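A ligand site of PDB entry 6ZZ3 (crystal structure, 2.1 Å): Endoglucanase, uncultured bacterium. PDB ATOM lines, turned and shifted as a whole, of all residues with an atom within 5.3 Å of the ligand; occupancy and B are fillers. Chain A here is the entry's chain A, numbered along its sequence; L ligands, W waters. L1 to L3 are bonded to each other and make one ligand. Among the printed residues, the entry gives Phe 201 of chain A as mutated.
O of Ser 207 is in hydrogen-bond range of O5 of LIG L1 (3.3 Å). O2 of LIG L1 sits at hydrogen-bond distance from NE2 of His 90 (3.1 Å). OE2 of Glu 135 lies close to O1 of LIG L1 (3.4 Å). OE2 of Glu 245 is covalently linked to C1 of LIG L1. An oxygen (O1) of LG3 L3 lies within hydrogen-bond range of the backbone NH (N) of Thr 15, at 3.0 Å. The side-chain amide nitrogen (ND2) of Asn 134 is in hydrogen-bond range of an oxygen (O1) of LIG L1 (3.3 Å). The indole nitrogen (NE1) of Trp 276 lies within hydrogen-bond range of an oxygen (O3) of LIG L1, 3.2 Å away. OH of Tyr 92 sits at hydrogen-bond distance from O2 of LIG L1, 3.4 Å away. O5 of LG2 L2 lies within hydrogen-bond range of OE2 of Glu 13, at 2.6 Å. OG1 of Thr 15 lies within hydrogen-bond range of O2 of LG3 L3, at 3.0 Å.
A ring nitrogen (NE2) of His 90 is in hydrogen-bond range of the side-chain amide nitrogen (ND2) of Asn 134, at 3.3 Å. The backbone carbonyl oxygen of Asn 134 sits at hydrogen-bond distance from the backbone NH of Tyr 92 (2.8 Å). The side-chain hydroxyl (OH) of Tyr 92 sits at hydrogen-bond distance from a ring nitrogen (NE2) of His 90 (3.4 Å). A ring nitrogen (ND1) of His 199 lies within hydrogen-bond range of the side-chain carboxylate (OE1) of Glu 245 (3.1 Å). The side-chain hydroxyl (OG) of Ser 207 sits at hydrogen-bond distance from the side-chain hydroxyl (OG) of Ser 209 (2.6 Å). The side-chain hydroxyl (OH) of Tyr 285 sits at hydrogen-bond distance from the indole nitrogen (NE1) of Trp 276, at 3.0 Å. OG1 of Thr 15 sits at hydrogen-bond distance from O of His 26 (2.6 Å). The side-chain carboxylate of Glu 135 is in hydrogen-bond range of a ring nitrogen (ND1) of His 199, 2.7 Å away.
CA of Phe 14 touches O1 of LG3 L3, 3.3 Å away. CE2 of Phe 201 touches O4 of LIG L1, at 3.2 Å. CZ3 of Trp 282 touches O5 of LG3 L3, at 3.9 Å. OH of Tyr 285 touches O3 of LIG L1 (3.7 Å). The nearest printed residue that does not touch the ligand is Gly 208 (4.3 Å).
Water W3 lies within hydrogen-bond range of O1 of LIG L1, OE2 of Glu 245 and OD1 of Asn 134. Water W2 lies within hydrogen-bond range of O5 of LG2 L2 (2.8 Å) and OH of Tyr 92 (2.9 Å). Water W5 lies within hydrogen-bond range of O2 of LG3 L3, OG1 of Thr 15 and O of His 26. Water W1 lies within hydrogen-bond range of the side-chain hydroxyl of Tyr 285 (2.6 Å), the backbone carbonyl oxygen of Gly 208 (2.7 Å) and an oxygen (O1) of LG2 L2 (3.3 Å).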
ATOM      1  N   GLU A  13     -16.544   2.880  -2.228  1.00  0.00           N
ATOM      2  CA  GLU A  13     -17.834   3.506  -2.487  1.00  0.00           C
ATOM      3  C   GLU A  13     -18.384   4.291  -1.292  1.00  0.00           C
ATOM      4  O   GLU A  13     -19.476   4.859  -1.395  1.00  0.00           O
ATOM      5  CB  GLU A  13     -18.862   2.443  -2.910  1.00  0.00           C
ATOM      6  CG  GLU A  13     -19.576   1.715  -1.736  1.00  0.00           C
ATOM      7  CD  GLU A  13     -18.707   0.694  -1.002  1.00  0.00           C
ATOM      8  OE1 GLU A  13     -17.483   0.647  -1.247  1.00  0.00           O
ATOM      9  OE2 GLU A  13     -19.253  -0.051  -0.158  1.00  0.00           O
ATOM     10  N   PHE A  14     -17.666   4.357  -0.182  1.00  0.00           N
ATOM     11  CA  PHE A  14     -18.178   4.958   1.043  1.00  0.00           C
ATOM     12  C   PHE A  14     -18.415   6.462   0.877  1.00  0.00           C
ATOM     13  O   PHE A  14     -17.867   7.119  -0.018  1.00  0.00           O
ATOM     14  CB  PHE A  14     -17.225   4.744   2.219  1.00  0.00           C
ATOM     15  CG  PHE A  14     -17.224   3.336   2.762  1.00  0.00           C
ATOM     16  CD1 PHE A  14     -17.966   2.325   2.161  1.00  0.00           C
ATOM     17  CD2 PHE A  14     -16.475   3.017   3.892  1.00  0.00           C
ATOM     18  CE1 PHE A  14     -17.964   1.033   2.654  1.00  0.00           C
ATOM     19  CE2 PHE A  14     -16.468   1.709   4.397  1.00  0.00           C
ATOM     20  CZ  PHE A  14     -17.220   0.730   3.772  1.00  0.00           C
ATOM     21  N   THR A  15     -19.256   6.995   1.773  1.00  0.00           N
ATOM     22  CA  THR A  15     -19.540   8.426   1.907  1.00  0.00           C
ATOM     23  C   THR A  15     -19.991   9.023   0.573  1.00  0.00           C
ATOM     24  O   THR A  15     -19.304   9.833  -0.048  1.00  0.00           O
ATOM     25  CB  THR A  15     -18.323   9.213   2.436  1.00  0.00           C
ATOM     26  OG1 THR A  15     -17.667   8.469   3.474  1.00  0.00           O
ATOM     27  CG2 THR A  15     -18.809  10.538   3.024  1.00  0.00           C
ATOM     28  N   GLY A  16     -21.149   8.559   0.113  1.00  0.00           N
ATOM     29  CA  GLY A  16     -21.695   9.015  -1.152  1.00  0.00           C
ATOM     30  C   GLY A  16     -21.939  10.514  -1.218  1.00  0.00           C
ATOM     31  O   GLY A  16     -22.005  11.084  -2.321  1.00  0.00           O
ATOM     32  N   HIS A  26     -12.899   9.942   3.039  1.00  0.00           N
ATOM     33  CA  HIS A  26     -14.288   9.553   2.806  1.00  0.00           C
ATOM     34  C   HIS A  26     -14.440   8.158   2.233  1.00  0.00           C
ATOM     35  O   HIS A  26     -15.462   7.512   2.478  1.00  0.00           O
ATOM     36  CB  HIS A  26     -14.957  10.547   1.855  1.00  0.00           C
ATOM     37  CG  HIS A  26     -14.670  11.973   2.176  1.00  0.00           C
ATOM     38  ND1 HIS A  26     -13.776  12.734   1.461  1.00  0.00           N
ATOM     39  CD2 HIS A  26     -15.160  12.781   3.153  1.00  0.00           C
ATOM     40  CE1 HIS A  26     -13.721  13.948   1.982  1.00  0.00           C
ATOM     41  NE2 HIS A  26     -14.544  14.004   3.002  1.00  0.00           N
ATOM     42  N   HIS A  90     -21.527   0.351  -7.843  1.00  0.00           N
ATOM     43  CA  HIS A  90     -22.388   0.259  -6.663  1.00  0.00           C
ATOM     44  C   HIS A  90     -23.349   1.455  -6.604  1.00  0.00           C
ATOM     45  O   HIS A  90     -23.304   2.266  -5.690  1.00  0.00           O
ATOM     46  CB  HIS A  90     -21.510   0.190  -5.417  1.00  0.00           C
ATOM     47  CG  HIS A  90     -22.133  -0.526  -4.243  1.00  0.00           C
ATOM     48  ND1 HIS A  90     -22.029  -1.892  -4.064  1.00  0.00           N
ATOM     49  CD2 HIS A  90     -22.830  -0.060  -3.183  1.00  0.00           C
ATOM     50  CE1 HIS A  90     -22.663  -2.232  -2.947  1.00  0.00           C
ATOM     51  NE2 HIS A  90     -23.154  -1.141  -2.398  1.00  0.00           N
ATOM     52  N   TYR A  92     -27.088   1.628  -7.569  1.00  0.00           N
ATOM     53  CA  TYR A  92     -28.539   1.545  -7.413  1.00  0.00           C
ATOM     54  C   TYR A  92     -29.268   2.074  -8.645  1.00  0.00           C
ATOM     55  O   TYR A  92     -30.375   2.603  -8.536  1.00  0.00           O
ATOM     56  CB  TYR A  92     -28.987   2.271  -6.131  1.00  0.00           C
ATOM     57  CG  TYR A  92     -28.179   1.856  -4.912  1.00  0.00           C
ATOM     58  CD1 TYR A  92     -28.559   0.747  -4.143  1.00  0.00           C
ATOM     59  CD2 TYR A  92     -26.992   2.503  -4.579  1.00  0.00           C
ATOM     60  CE1 TYR A  92     -27.821   0.355  -3.038  1.00  0.00           C
ATOM     61  CE2 TYR A  92     -26.250   2.116  -3.487  1.00  0.00           C
ATOM     62  CZ  TYR A  92     -26.664   1.034  -2.719  1.00  0.00           C
ATOM     63  OH  TYR A  92     -25.920   0.640  -1.621  1.00  0.00           O
ATOM     64  N   ASN A 134     -25.204  -2.385  -8.857  1.00  0.00           N
ATOM     65  CA  ASN A 134     -25.656  -2.873  -7.560  1.00  0.00           C
ATOM     66  C   ASN A 134     -27.071  -2.358  -7.282  1.00  0.00           C
ATOM     67  O   ASN A 134     -27.305  -1.156  -7.253  1.00  0.00           O
ATOM     68  CB  ASN A 134     -24.707  -2.415  -6.456  1.00  0.00           C
ATOM     69  CG  ASN A 134     -25.192  -2.817  -5.065  1.00  0.00           C
ATOM     70  OD1 ASN A 134     -25.106  -3.982  -4.692  1.00  0.00           O
ATOM     71  ND2 ASN A 134     -25.719  -1.847  -4.304  1.00  0.00           N
ATOM     72  N   GLU A 135     -28.011  -3.293  -7.097  1.00  0.00           N
ATOM     73  CA  GLU A 135     -29.323  -3.069  -6.509  1.00  0.00           C
ATOM     74  C   GLU A 135     -30.126  -1.926  -7.121  1.00  0.00           C
ATOM     75  O   GLU A 135     -30.299  -0.888  -6.489  1.00  0.00           O
ATOM     76  CB  GLU A 135     -29.182  -2.846  -4.996  1.00  0.00           C
ATOM     77  CG  GLU A 135     -28.738  -4.109  -4.252  1.00  0.00           C
ATOM     78  CD  GLU A 135     -28.606  -3.921  -2.749  1.00  0.00           C
ATOM     79  OE1 GLU A 135     -28.847  -2.800  -2.239  1.00  0.00           O
ATOM     80  OE2 GLU A 135     -28.245  -4.913  -2.090  1.00  0.00           O
ATOM     81  N   HIS A 199     -29.514 -10.855  -3.913  1.00  0.00           N
ATOM     82  CA  HIS A 199     -29.027 -10.490  -2.601  1.00  0.00           C
ATOM     83  C   HIS A 199     -30.001 -10.956  -1.541  1.00  0.00           C
ATOM     84  O   HIS A 199     -31.216 -10.985  -1.767  1.00  0.00           O
ATOM     85  CB  HIS A 199     -28.849  -8.982  -2.489  1.00  0.00           C
ATOM     86  CG  HIS A 199     -27.806  -8.423  -3.398  1.00  0.00           C
ATOM     87  ND1 HIS A 199     -27.496  -7.078  -3.438  1.00  0.00           N
ATOM     88  CD2 HIS A 199     -26.956  -9.026  -4.271  1.00  0.00           C
ATOM     89  CE1 HIS A 199     -26.519  -6.876  -4.305  1.00  0.00           C
ATOM     90  NE2 HIS A 199     -26.177  -8.041  -4.826  1.00  0.00           N
ATOM     91  N   PHE A 201     -30.505 -11.106   3.008  1.00  0.00           N
ATOM     92  CA  PHE A 201     -30.151 -11.056   4.411  1.00  0.00           C
ATOM     93  C   PHE A 201     -31.228 -11.801   5.185  1.00  0.00           C
ATOM     94  O   PHE A 201     -32.333 -12.010   4.670  1.00  0.00           O
ATOM     95  CB  PHE A 201     -30.049  -9.626   4.931  1.00  0.00           C
ATOM     96  CG  PHE A 201     -28.905  -8.860   4.352  1.00  0.00           C
ATOM     97  CD1 PHE A 201     -27.602  -9.096   4.756  1.00  0.00           C
ATOM     98  CD2 PHE A 201     -29.136  -7.900   3.375  1.00  0.00           C
ATOM     99  CE1 PHE A 201     -26.547  -8.379   4.213  1.00  0.00           C
ATOM    100  CE2 PHE A 201     -28.089  -7.180   2.821  1.00  0.00           C
ATOM    101  CZ  PHE A 201     -26.784  -7.408   3.253  1.00  0.00           C
ATOM    102  N   SER A 207     -33.418  -6.276   5.598  1.00  0.00           N
ATOM    103  CA  SER A 207     -32.604  -5.143   5.179  1.00  0.00           C
ATOM    104  C   SER A 207     -31.115  -5.333   5.470  1.00  0.00           C
ATOM    105  O   SER A 207     -30.295  -4.560   4.973  1.00  0.00           O
ATOM    106  CB  SER A 207     -33.086  -3.871   5.885  1.00  0.00           C
ATOM    107  OG  SER A 207     -32.752  -3.883   7.263  1.00  0.00           O
ATOM    108  N   GLY A 208     -30.743  -6.326   6.261  1.00  0.00           N
ATOM    109  CA  GLY A 208     -29.355  -6.467   6.621  1.00  0.00           C
ATOM    110  C   GLY A 208     -28.890  -5.477   7.667  1.00  0.00           C
ATOM    111  O   GLY A 208     -27.700  -5.420   7.960  1.00  0.00           O
ATOM    112  N   SER A 209     -29.819  -4.725   8.271  1.00  0.00           N
ATOM    113  CA  SER A 209     -29.441  -3.871   9.391  1.00  0.00           C
ATOM    114  C   SER A 209     -29.450  -4.625  10.708  1.00  0.00           C
ATOM    115  O   SER A 209     -28.794  -4.189  11.652  1.00  0.00           O
ATOM    116  CB  SER A 209     -30.371  -2.657   9.445  1.00  0.00           C
ATOM    117  OG  SER A 209     -31.721  -3.063   9.469  1.00  0.00           O
ATOM    118  N   GLU A 245     -24.514 -10.697  -2.294  1.00  0.00           N
ATOM    119  CA  GLU A 245     -24.512 -10.008  -1.010  1.00  0.00           C
ATOM    120  C   GLU A 245     -25.279 -10.826   0.028  1.00  0.00           C
ATOM    121  O   GLU A 245     -26.470 -11.070  -0.154  1.00  0.00           O
ATOM    122  CB  GLU A 245     -25.116  -8.614  -1.149  1.00  0.00           C
ATOM    123  CG  GLU A 245     -25.070  -7.784   0.119  1.00  0.00           C
ATOM    124  CD  GLU A 245     -26.047  -6.592   0.058  1.00  0.00           C
ATOM    125  OE1 GLU A 245     -27.223  -6.788  -0.325  1.00  0.00           O
ATOM    126  OE2 GLU A 245     -25.636  -5.470   0.402  1.00  0.00           O
ATOM    127  N   TRP A 276     -20.938 -10.341   2.643  1.00  0.00           N
ATOM    128  CA  TRP A 276     -20.975  -8.909   2.942  1.00  0.00           C
ATOM    129  C   TRP A 276     -20.783  -8.689   4.448  1.00  0.00           C
ATOM    130  O   TRP A 276     -21.681  -9.022   5.244  1.00  0.00           O
ATOM    131  CB  TRP A 276     -22.315  -8.310   2.492  1.00  0.00           C
ATOM    132  CG  TRP A 276     -22.326  -6.812   2.699  1.00  0.00           C
ATOM    133  CD1 TRP A 276     -22.716  -6.126   3.818  1.00  0.00           C
ATOM    134  CD2 TRP A 276     -21.844  -5.826   1.773  1.00  0.00           C
ATOM    135  NE1 TRP A 276     -22.538  -4.761   3.631  1.00  0.00           N
ATOM    136  CE2 TRP A 276     -22.011  -4.558   2.386  1.00  0.00           C
ATOM    137  CE3 TRP A 276     -21.309  -5.892   0.489  1.00  0.00           C
ATOM    138  CZ2 TRP A 276     -21.637  -3.371   1.742  1.00  0.00           C
ATOM    139  CZ3 TRP A 276     -20.955  -4.712  -0.158  1.00  0.00           C
ATOM    140  CH2 TRP A 276     -21.109  -3.462   0.477  1.00  0.00           C
ATOM    141  N   TRP A 282     -13.937  -0.662   8.054  1.00  0.00           N
ATOM    142  CA  TRP A 282     -15.307  -0.874   8.471  1.00  0.00           C
ATOM    143  C   TRP A 282     -15.548  -0.478   9.917  1.00  0.00           C
ATOM    144  O   TRP A 282     -16.708  -0.277  10.312  1.00  0.00           O
ATOM    145  CB  TRP A 282     -15.679  -2.348   8.308  1.00  0.00           C
ATOM    146  CG  TRP A 282     -16.322  -2.733   6.993  1.00  0.00           C
ATOM    147  CD1 TRP A 282     -15.873  -3.685   6.113  1.00  0.00           C
ATOM    148  CD2 TRP A 282     -17.564  -2.250   6.470  1.00  0.00           C
ATOM    149  NE1 TRP A 282     -16.750  -3.797   5.054  1.00  0.00           N
ATOM    150  CE2 TRP A 282     -17.789  -2.918   5.232  1.00  0.00           C
ATOM    151  CE3 TRP A 282     -18.498  -1.292   6.888  1.00  0.00           C
ATOM    152  CZ2 TRP A 282     -18.920  -2.673   4.445  1.00  0.00           C
ATOM    153  CZ3 TRP A 282     -19.622  -1.050   6.094  1.00  0.00           C
ATOM    154  CH2 TRP A 282     -19.817  -1.733   4.894  1.00  0.00           C
ATOM    155  N   TYR A 285     -18.596  -1.905  12.242  1.00  0.00           N
ATOM    156  CA  TYR A 285     -19.687  -2.442  11.433  1.00  0.00           C
ATOM    157  C   TYR A 285     -19.993  -3.875  11.819  1.00  0.00           C
ATOM    158  O   TYR A 285     -19.099  -4.726  11.839  1.00  0.00           O
ATOM    159  CB  TYR A 285     -19.318  -2.382   9.951  1.00  0.00           C
ATOM    160  CG  TYR A 285     -20.419  -2.796   9.017  1.00  0.00           C
ATOM    161  CD1 TYR A 285     -21.700  -2.237   9.113  1.00  0.00           C
ATOM    162  CD2 TYR A 285     -20.206  -3.763   8.034  1.00  0.00           C
ATOM    163  CE1 TYR A 285     -22.717  -2.623   8.255  1.00  0.00           C
ATOM    164  CE2 TYR A 285     -21.208  -4.147   7.174  1.00  0.00           C
ATOM    165  CZ  TYR A 285     -22.464  -3.587   7.296  1.00  0.00           C
ATOM    166  OH  TYR A 285     -23.460  -3.973   6.429  1.00  0.00           O
ATOM    167  N   LEU A 287     -21.594  -6.424  10.531  1.00  0.00           N
ATOM    168  CA  LEU A 287     -21.487  -7.531   9.589  1.00  0.00           C
ATOM    169  C   LEU A 287     -20.058  -7.729   9.096  1.00  0.00           C
ATOM    170  O   LEU A 287     -19.802  -8.678   8.346  1.00  0.00           O
ATOM    171  CB  LEU A 287     -22.428  -7.324   8.383  1.00  0.00           C
ATOM    172  CG  LEU A 287     -23.922  -7.131   8.704  1.00  0.00           C
ATOM    173  CD1 LEU A 287     -24.780  -7.249   7.456  1.00  0.00           C
ATOM    174  CD2 LEU A 287     -24.385  -8.104   9.795  1.00  0.00           C
HETATM  175  C1  LIG L   1     -26.554  -4.446   0.385  1.00  0.00           C
HETATM  176  C2  LIG L   1     -25.907  -3.144  -0.070  1.00  0.00           C
HETATM  177  C3  LIG L   1     -24.868  -2.728   0.889  1.00  0.00           C
HETATM  178  C4  LIG L   1     -25.440  -2.573   2.292  1.00  0.00           C
HETATM  179  C5  LIG L   1     -26.059  -3.912   2.687  1.00  0.00           C
HETATM  180  C6  LIG L   1     -26.620  -3.875   4.063  1.00  0.00           C
HETATM  181  O1  LIG L   1     -25.363  -3.350  -1.375  1.00  0.00           O
HETATM  182  O2  LIG L   1     -24.301  -1.467   0.428  1.00  0.00           O
HETATM  183  O3  LIG L   1     -24.419  -2.203   3.267  1.00  0.00           O
HETATM  184  O4  LIG L   1     -27.133  -4.284   1.748  1.00  0.00           O
HETATM  185  O5  LIG L   1     -27.585  -2.879   4.146  1.00  0.00           O
HETATM  186  C1  LG2 L   2     -24.025  -0.491   4.889  1.00  0.00           C
HETATM  187  C2  LG2 L   2     -23.605   0.930   5.065  1.00  0.00           C
HETATM  188  C3  LG2 L   2     -22.446   1.303   4.222  1.00  0.00           C
HETATM  189  C4  LG2 L   2     -22.723   0.951   2.760  1.00  0.00           C
HETATM  190  C5  LG2 L   2     -21.521   1.179   1.875  1.00  0.00           C
HETATM  191  C6  LG2 L   2     -24.268  -0.832   3.428  1.00  0.00           C
HETATM  192  O1  LG2 L   2     -25.229  -0.736   5.629  1.00  0.00           O
HETATM  193  O2  LG2 L   2     -23.282   1.156   6.478  1.00  0.00           O
HETATM  194  O3  LG2 L   2     -22.238   2.729   4.280  1.00  0.00           O
HETATM  195  O4  LG2 L   2     -23.068  -0.476   2.650  1.00  0.00           O
HETATM  196  O5  LG2 L   2     -21.718   0.478   0.635  1.00  0.00           O
HETATM  197  C1  LG3 L   3     -20.743   4.529   4.504  1.00  0.00           C
HETATM  198  C2  LG3 L   3     -19.460   4.910   5.130  1.00  0.00           C
HETATM  199  C3  LG3 L   3     -19.570   4.707   6.612  1.00  0.00           C
HETATM  200  C4  LG3 L   3     -19.839   3.243   6.959  1.00  0.00           C
HETATM  201  C5  LG3 L   3     -20.059   3.115   8.430  1.00  0.00           C
HETATM  202  C6  LG3 L   3     -21.016   3.047   4.794  1.00  0.00           C
HETATM  203  O1  LG3 L   3     -20.725   4.752   3.068  1.00  0.00           O
HETATM  204  O2  LG3 L   3     -19.125   6.291   4.888  1.00  0.00           O
HETATM  205  O3  LG3 L   3     -18.341   5.106   7.233  1.00  0.00           O
HETATM  206  O4  LG3 L   3     -21.049   2.772   6.268  1.00  0.00           O
HETATM  207  O5  LG3 L   3     -20.343   1.772   8.723  1.00  0.00           O
HETATM  208  O   HOH W   1     -25.855  -3.497   7.348  1.00  0.00           O
HETATM  209  O   HOH W   2     -23.576   2.034  -0.668  1.00  0.00           O
HETATM  210  O   HOH W   3     -24.001  -5.429  -2.048  1.00  0.00           O
HETATM  211  O   HOH W   4     -25.705   0.628   8.276  1.00  0.00           O
HETATM  212  O   HOH W   5     -16.337   6.516   5.533  1.00  0.00           O
